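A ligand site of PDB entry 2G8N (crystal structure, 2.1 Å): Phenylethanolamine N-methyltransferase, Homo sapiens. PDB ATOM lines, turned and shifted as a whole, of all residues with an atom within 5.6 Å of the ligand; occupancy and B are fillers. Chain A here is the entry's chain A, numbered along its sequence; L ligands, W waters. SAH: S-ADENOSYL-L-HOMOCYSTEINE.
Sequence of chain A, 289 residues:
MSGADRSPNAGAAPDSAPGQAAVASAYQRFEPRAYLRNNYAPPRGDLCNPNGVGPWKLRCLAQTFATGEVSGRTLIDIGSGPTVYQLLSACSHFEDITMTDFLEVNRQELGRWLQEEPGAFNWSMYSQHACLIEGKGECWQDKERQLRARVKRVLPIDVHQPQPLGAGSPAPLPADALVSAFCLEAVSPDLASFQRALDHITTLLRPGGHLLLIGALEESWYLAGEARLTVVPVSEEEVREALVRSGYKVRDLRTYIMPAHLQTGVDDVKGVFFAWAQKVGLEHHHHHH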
ATOM      1  N   VAL A  23       3.063 -15.559  10.512  1.00  0.00           N
ATOM      2  CA  VAL A  23       3.123 -16.859  11.253  1.00  0.00           C
ATOM      3  C   VAL A  23       2.985 -18.028  10.267  1.00  0.00           C
ATOM      4  O   VAL A  23       3.745 -18.991  10.329  1.00  0.00           O
ATOM      5  CB  VAL A  23       1.995 -16.949  12.346  1.00  0.00           C
ATOM      6  CG1 VAL A  23       2.108 -15.786  13.314  1.00  0.00           C
ATOM      7  CG2 VAL A  23       0.606 -16.962  11.703  1.00  0.00           C
ATOM      8  N   TYR A  27       4.780 -21.614  10.278  1.00  0.00           N
ATOM      9  CA  TYR A  27       4.035 -22.866  10.357  1.00  0.00           C
ATOM     10  C   TYR A  27       4.321 -23.826   9.211  1.00  0.00           C
ATOM     11  O   TYR A  27       3.889 -24.968   9.229  1.00  0.00           O
ATOM     12  CB  TYR A  27       2.538 -22.589  10.485  1.00  0.00           C
ATOM     13  CG  TYR A  27       2.139 -22.340  11.912  1.00  0.00           C
ATOM     14  CD1 TYR A  27       1.893 -21.050  12.383  1.00  0.00           C
ATOM     15  CD2 TYR A  27       2.064 -23.397  12.824  1.00  0.00           C
ATOM     16  CE1 TYR A  27       1.602 -20.819  13.718  1.00  0.00           C
ATOM     17  CE2 TYR A  27       1.775 -23.181  14.151  1.00  0.00           C
ATOM     18  CZ  TYR A  27       1.541 -21.905  14.591  1.00  0.00           C
ATOM     19  OH  TYR A  27       1.266 -21.690  15.920  1.00  0.00           O
ATOM     20  N   PHE A  30       6.375 -26.606  10.648  1.00  0.00           N
ATOM     21  CA  PHE A  30       5.743 -27.358  11.736  1.00  0.00           C
ATOM     22  C   PHE A  30       5.732 -28.890  11.532  1.00  0.00           C
ATOM     23  O   PHE A  30       5.080 -29.389  10.615  1.00  0.00           O
ATOM     24  CB  PHE A  30       4.306 -26.859  11.904  1.00  0.00           C
ATOM     25  CG  PHE A  30       3.604 -27.392  13.124  1.00  0.00           C
ATOM     26  CD1 PHE A  30       3.502 -26.611  14.274  1.00  0.00           C
ATOM     27  CD2 PHE A  30       2.978 -28.637  13.095  1.00  0.00           C
ATOM     28  CE1 PHE A  30       2.770 -27.061  15.379  1.00  0.00           C
ATOM     29  CE2 PHE A  30       2.240 -29.090  14.192  1.00  0.00           C
ATOM     30  CZ  PHE A  30       2.145 -28.298  15.346  1.00  0.00           C
ATOM     31  N   TYR A  35       5.849 -32.168  17.469  1.00  0.00           N
ATOM     32  CA  TYR A  35       4.884 -31.437  18.293  1.00  0.00           C
ATOM     33  C   TYR A  35       4.252 -32.381  19.322  1.00  0.00           C
ATOM     34  O   TYR A  35       4.125 -32.057  20.506  1.00  0.00           O
ATOM     35  CB  TYR A  35       3.786 -30.834  17.413  1.00  0.00           C
ATOM     36  CG  TYR A  35       2.704 -30.119  18.202  1.00  0.00           C
ATOM     37  CD1 TYR A  35       2.936 -28.855  18.733  1.00  0.00           C
ATOM     38  CD2 TYR A  35       1.477 -30.733  18.457  1.00  0.00           C
ATOM     39  CE1 TYR A  35       1.965 -28.204  19.499  1.00  0.00           C
ATOM     40  CE2 TYR A  35       0.492 -30.091  19.225  1.00  0.00           C
ATOM     41  CZ  TYR A  35       0.748 -28.836  19.741  1.00  0.00           C
ATOM     42  OH  TYR A  35      -0.194 -28.200  20.503  1.00  0.00           O
ATOM     43  N   TYR A  40       2.821 -34.246  24.210  1.00  0.00           N
ATOM     44  CA  TYR A  40       1.899 -35.277  24.623  1.00  0.00           C
ATOM     45  C   TYR A  40       2.530 -36.593  25.000  1.00  0.00           C
ATOM     46  O   TYR A  40       1.848 -37.572  25.232  1.00  0.00           O
ATOM     47  CB  TYR A  40       0.811 -35.420  23.554  1.00  0.00           C
ATOM     48  CG  TYR A  40       0.010 -34.130  23.452  1.00  0.00           C
ATOM     49  CD1 TYR A  40       0.334 -33.153  22.508  1.00  0.00           C
ATOM     50  CD2 TYR A  40      -1.048 -33.871  24.332  1.00  0.00           C
ATOM     51  CE1 TYR A  40      -0.366 -31.955  22.442  1.00  0.00           C
ATOM     52  CE2 TYR A  40      -1.764 -32.667  24.276  1.00  0.00           C
ATOM     53  CZ  TYR A  40      -1.413 -31.715  23.331  1.00  0.00           C
ATOM     54  OH  TYR A  40      -2.105 -30.520  23.260  1.00  0.00           O
ATOM     55  N   ASP A  77     -14.115 -28.239  16.199  1.00  0.00           N
ATOM     56  CA  ASP A  77     -12.859 -28.114  16.918  1.00  0.00           C
ATOM     57  C   ASP A  77     -11.952 -27.250  16.035  1.00  0.00           C
ATOM     58  O   ASP A  77     -11.585 -27.643  14.915  1.00  0.00           O
ATOM     59  CB  ASP A  77     -12.232 -29.495  17.151  1.00  0.00           C
ATOM     60  CG  ASP A  77     -10.928 -29.429  17.920  1.00  0.00           C
ATOM     61  OD1 ASP A  77     -10.838 -28.587  18.829  1.00  0.00           O
ATOM     62  OD2 ASP A  77      -9.997 -30.217  17.622  1.00  0.00           O
ATOM     63  N   ILE A  78     -11.606 -26.074  16.563  1.00  0.00           N
ATOM     64  CA  ILE A  78     -10.785 -25.078  15.858  1.00  0.00           C
ATOM     65  C   ILE A  78      -9.279 -25.230  16.060  1.00  0.00           C
ATOM     66  O   ILE A  78      -8.781 -25.064  17.185  1.00  0.00           O
ATOM     67  CB  ILE A  78     -11.151 -23.645  16.329  1.00  0.00           C
ATOM     68  CG1 ILE A  78     -12.675 -23.425  16.274  1.00  0.00           C
ATOM     69  CG2 ILE A  78     -10.375 -22.608  15.510  1.00  0.00           C
ATOM     70  CD1 ILE A  78     -13.292 -23.675  14.915  1.00  0.00           C
ATOM     71  N   GLY A  79      -8.566 -25.503  14.981  1.00  0.00           N
ATOM     72  CA  GLY A  79      -7.129 -25.662  15.080  1.00  0.00           C
ATOM     73  C   GLY A  79      -6.726 -26.924  15.829  1.00  0.00           C
ATOM     74  O   GLY A  79      -5.861 -26.887  16.689  1.00  0.00           O
ATOM     75  N   SER A  80      -7.356 -28.026  15.456  1.00  0.00           N
ATOM     76  CA  SER A  80      -7.123 -29.335  16.064  1.00  0.00           C
ATOM     77  C   SER A  80      -5.678 -29.791  16.019  1.00  0.00           C
ATOM     78  O   SER A  80      -5.257 -30.595  16.857  1.00  0.00           O
ATOM     79  CB  SER A  80      -7.967 -30.395  15.352  1.00  0.00           C
ATOM     80  OG  SER A  80      -9.310 -29.996  15.219  1.00  0.00           O
ATOM     81  N   GLY A  81      -4.918 -29.295  15.047  1.00  0.00           N
ATOM     82  CA  GLY A  81      -3.547 -29.755  14.929  1.00  0.00           C
ATOM     83  C   GLY A  81      -3.604 -31.278  14.784  1.00  0.00           C
ATOM     84  O   GLY A  81      -4.564 -31.809  14.201  1.00  0.00           O
ATOM     85  N   PRO A  82      -2.597 -32.012  15.308  1.00  0.00           N
ATOM     86  CA  PRO A  82      -2.562 -33.485  15.218  1.00  0.00           C
ATOM     87  C   PRO A  82      -3.068 -34.163  16.498  1.00  0.00           C
ATOM     88  O   PRO A  82      -2.651 -35.286  16.798  1.00  0.00           O
ATOM     89  CB  PRO A  82      -1.073 -33.753  15.014  1.00  0.00           C
ATOM     90  CG  PRO A  82      -0.472 -32.754  16.006  1.00  0.00           C
ATOM     91  CD  PRO A  82      -1.325 -31.490  15.836  1.00  0.00           C
ATOM     92  N   THR A  83      -3.956 -33.518  17.242  1.00  0.00           N
ATOM     93  CA  THR A  83      -4.416 -34.108  18.504  1.00  0.00           C
ATOM     94  C   THR A  83      -5.915 -34.364  18.572  1.00  0.00           C
ATOM     95  O   THR A  83      -6.701 -33.671  17.929  1.00  0.00           O
ATOM     96  CB  THR A  83      -4.040 -33.207  19.725  1.00  0.00           C
ATOM     97  OG1 THR A  83      -4.855 -32.027  19.742  1.00  0.00           O
ATOM     98  CG2 THR A  83      -2.575 -32.806  19.655  1.00  0.00           C
ATOM     99  N   TYR A  85      -7.274 -35.583  21.949  1.00  0.00           N
ATOM    100  CA  TYR A  85      -7.607 -35.634  23.384  1.00  0.00           C
ATOM    101  C   TYR A  85      -8.666 -34.607  23.772  1.00  0.00           C
ATOM    102  O   TYR A  85      -9.448 -34.846  24.676  1.00  0.00           O
ATOM    103  CB  TYR A  85      -6.362 -35.378  24.221  1.00  0.00           C
ATOM    104  CG  TYR A  85      -5.965 -33.919  24.216  1.00  0.00           C
ATOM    105  CD1 TYR A  85      -6.514 -33.038  25.135  1.00  0.00           C
ATOM    106  CD2 TYR A  85      -5.117 -33.411  23.237  1.00  0.00           C
ATOM    107  CE1 TYR A  85      -6.234 -31.672  25.097  1.00  0.00           C
ATOM    108  CE2 TYR A  85      -4.818 -32.038  23.169  1.00  0.00           C
ATOM    109  CZ  TYR A  85      -5.386 -31.179  24.110  1.00  0.00           C
ATOM    110  OH  TYR A  85      -5.130 -29.832  24.047  1.00  0.00           O
ATOM    111  N   GLN A  86      -8.679 -33.474  23.085  1.00  0.00           N
ATOM    112  CA  GLN A  86      -9.615 -32.398  23.384  1.00  0.00           C
ATOM    113  C   GLN A  86     -11.049 -32.770  23.058  1.00  0.00           C
ATOM    114  O   GLN A  86     -11.977 -32.070  23.454  1.00  0.00           O
ATOM    115  CB  GLN A  86      -9.217 -31.090  22.652  1.00  0.00           C
ATOM    116  CG  GLN A  86      -9.280 -31.144  21.129  1.00  0.00           C
ATOM    117  CD  GLN A  86      -8.005 -31.648  20.479  1.00  0.00           C
ATOM    118  OE1 GLN A  86      -7.247 -32.428  21.070  1.00  0.00           O
ATOM    119  NE2 GLN A  86      -7.766 -31.216  19.237  1.00  0.00           N
ATOM    120  N   ASP A 101      -7.826 -27.650  10.850  1.00  0.00           N
ATOM    121  CA  ASP A 101      -6.474 -27.145  10.989  1.00  0.00           C
ATOM    122  C   ASP A 101      -5.928 -26.495   9.729  1.00  0.00           C
ATOM    123  O   ASP A 101      -6.221 -26.910   8.604  1.00  0.00           O
ATOM    124  CB  ASP A 101      -5.491 -28.194  11.467  1.00  0.00           C
ATOM    125  CG  ASP A 101      -4.269 -27.555  12.122  1.00  0.00           C
ATOM    126  OD1 ASP A 101      -4.458 -26.918  13.182  1.00  0.00           O
ATOM    127  OD2 ASP A 101      -3.156 -27.661  11.567  1.00  0.00           O
ATOM    128  N   PHE A 102      -5.114 -25.468   9.946  1.00  0.00           N
ATOM    129  CA  PHE A 102      -4.507 -24.716   8.877  1.00  0.00           C
ATOM    130  C   PHE A 102      -3.521 -25.526   8.053  1.00  0.00           C
ATOM    131  O   PHE A 102      -3.420 -25.319   6.846  1.00  0.00           O
ATOM    132  CB  PHE A 102      -3.794 -23.526   9.483  1.00  0.00           C
ATOM    133  CG  PHE A 102      -3.190 -22.609   8.487  1.00  0.00           C
ATOM    134  CD1 PHE A 102      -3.988 -21.787   7.712  1.00  0.00           C
ATOM    135  CD2 PHE A 102      -1.808 -22.586   8.295  1.00  0.00           C
ATOM    136  CE1 PHE A 102      -3.426 -20.940   6.748  1.00  0.00           C
ATOM    137  CE2 PHE A 102      -1.233 -21.748   7.338  1.00  0.00           C
ATOM    138  CZ  PHE A 102      -2.045 -20.926   6.561  1.00  0.00           C
ATOM    139  N   LEU A 103      -2.794 -26.436   8.692  1.00  0.00           N
ATOM    140  CA  LEU A 103      -1.780 -27.233   8.000  1.00  0.00           C
ATOM    141  C   LEU A 103      -2.280 -28.558   7.477  1.00  0.00           C
ATOM    142  O   LEU A 103      -2.967 -29.293   8.178  1.00  0.00           O
ATOM    143  CB  LEU A 103      -0.585 -27.484   8.923  1.00  0.00           C
ATOM    144  CG  LEU A 103       0.171 -26.270   9.446  1.00  0.00           C
ATOM    145  CD1 LEU A 103       1.349 -26.677  10.335  1.00  0.00           C
ATOM    146  CD2 LEU A 103       0.666 -25.458   8.243  1.00  0.00           C
ATOM    147  N   ASN A 106      -1.060 -31.628   9.375  1.00  0.00           N
ATOM    148  CA  ASN A 106      -1.769 -31.983  10.598  1.00  0.00           C
ATOM    149  C   ASN A 106      -3.037 -32.734  10.247  1.00  0.00           C
ATOM    150  O   ASN A 106      -3.367 -33.746  10.892  1.00  0.00           O
ATOM    151  CB  ASN A 106      -2.120 -30.739  11.435  1.00  0.00           C
ATOM    152  CG  ASN A 106      -0.943 -30.241  12.259  1.00  0.00           C
ATOM    153  OD1 ASN A 106      -0.138 -31.050  12.745  1.00  0.00           O
ATOM    154  ND2 ASN A 106      -0.830 -28.926  12.439  1.00  0.00           N
ATOM    155  N   ILE A 157      -8.747 -24.570   7.758  1.00  0.00           N
ATOM    156  CA  ILE A 157      -9.350 -23.427   8.420  1.00  0.00           C
ATOM    157  C   ILE A 157      -8.252 -22.393   8.610  1.00  0.00           C
ATOM    158  O   ILE A 157      -7.067 -22.732   8.578  1.00  0.00           O
ATOM    159  CB  ILE A 157      -9.963 -23.854   9.794  1.00  0.00           C
ATOM    160  CG1 ILE A 157     -10.660 -22.677  10.464  1.00  0.00           C
ATOM    161  CG2 ILE A 157      -8.871 -24.430  10.709  1.00  0.00           C
ATOM    162  CD1 ILE A 157     -11.461 -23.074  11.722  1.00  0.00           C
ATOM    163  N   ASP A 158      -8.663 -21.139   8.748  1.00  0.00           N
ATOM    164  CA  ASP A 158      -7.735 -20.020   8.973  1.00  0.00           C
ATOM    165  C   ASP A 158      -8.491 -19.016   9.808  1.00  0.00           C
ATOM    166  O   ASP A 158      -9.344 -18.299   9.301  1.00  0.00           O
ATOM    167  CB  ASP A 158      -7.318 -19.344   7.671  1.00  0.00           C
ATOM    168  CG  ASP A 158      -6.305 -18.232   7.897  1.00  0.00           C
ATOM    169  OD1 ASP A 158      -6.118 -17.792   9.057  1.00  0.00           O
ATOM    170  OD2 ASP A 158      -5.697 -17.782   6.890  1.00  0.00           O
ATOM    171  N   VAL A 159      -8.159 -18.971  11.096  1.00  0.00           N
ATOM    172  CA  VAL A 159      -8.829 -18.071  12.009  1.00  0.00           C
ATOM    173  C   VAL A 159      -8.588 -16.613  11.703  1.00  0.00           C
ATOM    174  O   VAL A 159      -9.250 -15.737  12.273  1.00  0.00           O
ATOM    175  CB  VAL A 159      -8.428 -18.388  13.461  1.00  0.00           C
ATOM    176  CG1 VAL A 159      -8.900 -19.790  13.822  1.00  0.00           C
ATOM    177  CG2 VAL A 159      -6.924 -18.289  13.610  1.00  0.00           C
ATOM    178  N   HIS A 160      -7.629 -16.328  10.814  1.00  0.00           N
ATOM    179  CA  HIS A 160      -7.351 -14.942  10.452  1.00  0.00           C
ATOM    180  C   HIS A 160      -8.403 -14.402   9.467  1.00  0.00           C
ATOM    181  O   HIS A 160      -8.540 -13.189   9.298  1.00  0.00           O
ATOM    182  CB  HIS A 160      -5.966 -14.805   9.830  1.00  0.00           C
ATOM    183  CG  HIS A 160      -4.844 -15.182  10.752  1.00  0.00           C
ATOM    184  ND1 HIS A 160      -4.823 -14.807  12.079  1.00  0.00           N
ATOM    185  CD2 HIS A 160      -3.701 -15.869  10.527  1.00  0.00           C
ATOM    186  CE1 HIS A 160      -3.710 -15.249  12.635  1.00  0.00           C
ATOM    187  NE2 HIS A 160      -3.009 -15.898  11.721  1.00  0.00           N
ATOM    188  N   ALA A 181      -8.121 -25.557  21.302  1.00  0.00           N
ATOM    189  CA  ALA A 181      -7.054 -25.699  22.270  1.00  0.00           C
ATOM    190  C   ALA A 181      -5.727 -25.288  21.708  1.00  0.00           C
ATOM    191  O   ALA A 181      -5.288 -25.846  20.700  1.00  0.00           O
ATOM    192  CB  ALA A 181      -6.966 -27.165  22.746  1.00  0.00           C
ATOM    193  N   PHE A 182      -5.110 -24.300  22.361  1.00  0.00           N
ATOM    194  CA  PHE A 182      -3.781 -23.807  22.005  1.00  0.00           C
ATOM    195  C   PHE A 182      -3.622 -23.195  20.611  1.00  0.00           C
ATOM    196  O   PHE A 182      -2.496 -23.042  20.120  1.00  0.00           O
ATOM    197  CB  PHE A 182      -2.774 -24.946  22.166  1.00  0.00           C
ATOM    198  CG  PHE A 182      -2.684 -25.486  23.575  1.00  0.00           C
ATOM    199  CD1 PHE A 182      -3.048 -26.800  23.858  1.00  0.00           C
ATOM    200  CD2 PHE A 182      -2.199 -24.676  24.612  1.00  0.00           C
ATOM    201  CE1 PHE A 182      -2.927 -27.321  25.169  1.00  0.00           C
ATOM    202  CE2 PHE A 182      -2.077 -25.188  25.919  1.00  0.00           C
ATOM    203  CZ  PHE A 182      -2.442 -26.503  26.202  1.00  0.00           C
ATOM    204  N   CYS A 183      -4.716 -22.819  19.986  1.00  0.00           N
ATOM    205  CA  CYS A 183      -4.624 -22.251  18.650  1.00  0.00           C
ATOM    206  C   CYS A 183      -4.436 -20.729  18.572  1.00  0.00           C
ATOM    207  O   CYS A 183      -3.379 -20.246  18.168  1.00  0.00           O
ATOM    208  CB  CYS A 183      -5.860 -22.628  17.839  1.00  0.00           C
ATOM    209  SG  CYS A 183      -5.823 -22.068  16.110  1.00  0.00           S
ATOM    210  N   ALA A 186      -1.374 -18.925  19.661  1.00  0.00           N
ATOM    211  CA  ALA A 186      -0.246 -19.466  18.901  1.00  0.00           C
ATOM    212  C   ALA A 186      -0.178 -19.026  17.446  1.00  0.00           C
ATOM    213  O   ALA A 186       0.778 -19.361  16.743  1.00  0.00           O
ATOM    214  CB  ALA A 186      -0.240 -21.004  18.979  1.00  0.00           C
ATOM    215  N   VAL A 187      -1.194 -18.303  16.973  1.00  0.00           N
ATOM    216  CA  VAL A 187      -1.181 -17.828  15.587  1.00  0.00           C
ATOM    217  C   VAL A 187      -1.417 -16.315  15.554  1.00  0.00           C
ATOM    218  O   VAL A 187      -1.631 -15.739  14.493  1.00  0.00           O
ATOM    219  CB  VAL A 187      -2.261 -18.538  14.728  1.00  0.00           C
ATOM    220  CG1 VAL A 187      -2.187 -20.040  14.950  1.00  0.00           C
ATOM    221  CG2 VAL A 187      -3.650 -18.017  15.075  1.00  0.00           C
ATOM    222  N   TYR A 222       7.323 -21.639  21.152  1.00  0.00           N
ATOM    223  CA  TYR A 222       7.321 -23.095  21.364  1.00  0.00           C
ATOM    224  C   TYR A 222       7.912 -23.664  20.094  1.00  0.00           C
ATOM    225  O   TYR A 222       7.890 -23.000  19.048  1.00  0.00           O
ATOM    226  CB  TYR A 222       5.916 -23.673  21.613  1.00  0.00           C
ATOM    227  CG  TYR A 222       5.000 -23.735  20.417  1.00  0.00           C
ATOM    228  CD1 TYR A 222       4.789 -24.943  19.769  1.00  0.00           C
ATOM    229  CD2 TYR A 222       4.316 -22.602  19.965  1.00  0.00           C
ATOM    230  CE1 TYR A 222       3.888 -25.025  18.703  1.00  0.00           C
ATOM    231  CE2 TYR A 222       3.420 -22.680  18.907  1.00  0.00           C
ATOM    232  CZ  TYR A 222       3.218 -23.910  18.286  1.00  0.00           C
ATOM    233  OH  TYR A 222       2.316 -24.028  17.261  1.00  0.00           O
HETATM  234  N   SAH L   1      -5.133 -28.079  19.146  1.00  0.00           N
HETATM  235  CA  SAH L   1      -3.888 -28.844  19.204  1.00  0.00           C
HETATM  236  CB  SAH L   1      -2.789 -28.103  18.403  1.00  0.00           C
HETATM  237  CG  SAH L   1      -2.462 -26.679  18.891  1.00  0.00           C
HETATM  238  SD  SAH L   1      -0.914 -26.034  18.185  1.00  0.00           S
HETATM  239  C   SAH L   1      -3.452 -29.107  20.660  1.00  0.00           C
HETATM  240  O   SAH L   1      -2.274 -29.464  20.880  1.00  0.00           O
HETATM  241  OXT SAH L   1      -4.286 -28.957  21.564  1.00  0.00           O
HETATM  242  C5' SAH L   1      -1.557 -24.682  17.127  1.00  0.00           C
HETATM  243  C4' SAH L   1      -2.294 -25.137  15.875  1.00  0.00           C
HETATM  244  O4' SAH L   1      -2.856 -24.019  15.120  1.00  0.00           O
HETATM  245  C3' SAH L   1      -1.494 -25.967  14.872  1.00  0.00           C
HETATM  246  O3' SAH L   1      -2.209 -27.160  14.575  1.00  0.00           O
HETATM  247  C2' SAH L   1      -1.378 -25.034  13.669  1.00  0.00           C
HETATM  248  O2' SAH L   1      -1.237 -25.693  12.429  1.00  0.00           O
HETATM  249  C1' SAH L   1      -2.694 -24.281  13.739  1.00  0.00           C
HETATM  250  N9  SAH L   1      -2.759 -23.032  12.982  1.00  0.00           N
HETATM  251  C8  SAH L   1      -1.696 -22.269  12.441  1.00  0.00           C
HETATM  252  N7  SAH L   1      -2.089 -21.209  11.788  1.00  0.00           N
HETATM  253  C5  SAH L   1      -3.472 -21.267  11.900  1.00  0.00           C
HETATM  254  C6  SAH L   1      -4.443 -20.380  11.382  1.00  0.00           C
HETATM  255  N6  SAH L   1      -4.153 -19.280  10.682  1.00  0.00           N
HETATM  256  N1  SAH L   1      -5.751 -20.670  11.631  1.00  0.00           N
HETATM  257  C2  SAH L   1      -6.038 -21.795  12.351  1.00  0.00           C
HETATM  258  N3  SAH L   1      -5.199 -22.695  12.885  1.00  0.00           N
HETATM  259  C4  SAH L   1      -3.901 -22.369  12.618  1.00  0.00           C
HETATM  260  O   HOH W   1      -8.165 -27.483  19.044  1.00  0.00           O
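O of the ligand lies within hydrogen-bond range of OH of Tyr 35 (2.5 Å).
O of the ligand is in hydrogen-bond range of OH of Tyr 40 (2.6 Å).
The side-chain carboxylate (OD1) of Asp 101 sits at hydrogen-bond distance from an oxygen (O3') of the ligand.
O of Ala 181 sits at hydrogen-bond distance from N of the ligand (2.7 Å).
OH of Tyr 85 is in hydrogen-bond range of OXT of the ligand (2.8 Å).
A nitrogen (N) of the ligand sits at hydrogen-bond distance from the backbone carbonyl oxygen (O) of Gly 79 (2.8 Å).
The backbone NH of Gly 81 sits close to an oxygen (O3') of the ligand (3.5 Å).
A nitrogen (N6) of the ligand is in hydrogen-bond range of the side-chain carboxylate (OD1) of Asp 158 (3.0 Å).
A nitrogen (N1) of the ligand is in hydrogen-bond range of the backbone NH of Val 159, 3.0 Å away.
The side-chain amide nitrogen (ND2) of Asn 106 lies within hydrogen-bond range of an oxygen (O3') of the ligand (3.1 Å).
The backbone carbonyl oxygen (O) of Ser 80 sits close to a nitrogen (N) of the ligand (3.4 Å).
A nitrogen (N3) of the ligand is in hydrogen-bond range of the side-chain sulfur of Cys 183 (3.3 Å).
The side-chain hydroxyl of Tyr 40 sits close to the side-chain hydroxyl of Tyr 85, at 3.2 Å.
The side-chain carboxylate (OD1) of Asp 101 lies within hydrogen-bond range of the backbone NH (N) of Gly 81, at 3.1 Å.
The side-chain amide nitrogen (ND2) of Asn 106 is in hydrogen-bond range of the side-chain carboxylate (OD2) of Asp 101 (2.8 Å).
N of Leu 103 lies within hydrogen-bond range of OD2 of Asp 101.
OD1 of Asp 158 lies within hydrogen-bond range of N of His 160, at 2.7 Å.
The side-chain hydroxyl (OG) of Ser 80 lies within hydrogen-bond range of the side-chain carboxylate (OD2) of Asp 77 (2.5 Å).
A ring nitrogen (NE2) of His 160 lies close to the backbone carbonyl oxygen (O) of Val 187 (3.1 Å).
The side-chain hydroxyl (OH) of Tyr 222 is in hydrogen-bond range of the side-chain hydroxyl (OH) of Tyr 27 (2.9 Å).
Residues that only touch the ligand: Tyr 27 (3.7 Å), Thr 83 (3.4 Å), Phe 102 (3.3 Å), Leu 103 (3.3 Å), Ile 157 (3.9 Å), His 160 (3.4 Å), Phe 182 (3.4 Å), Val 187 (3.4 Å) and Tyr 222 (3.9 Å).
Within 4 Å of the ligand: Tyr 27, Tyr 35, Tyr 40, Gly 79, Ser 80, Gly 81, Thr 83, Tyr 85, Asp 101, Phe 102, Leu 103, Asn 106, Ile 157, Asp 158, Val 159, His 160, Ala 181, Phe 182, Cys 183, Val 187 and Tyr 222.
The nearest printed residue that does not touch the ligand is Gln 86 (4.1 Å).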
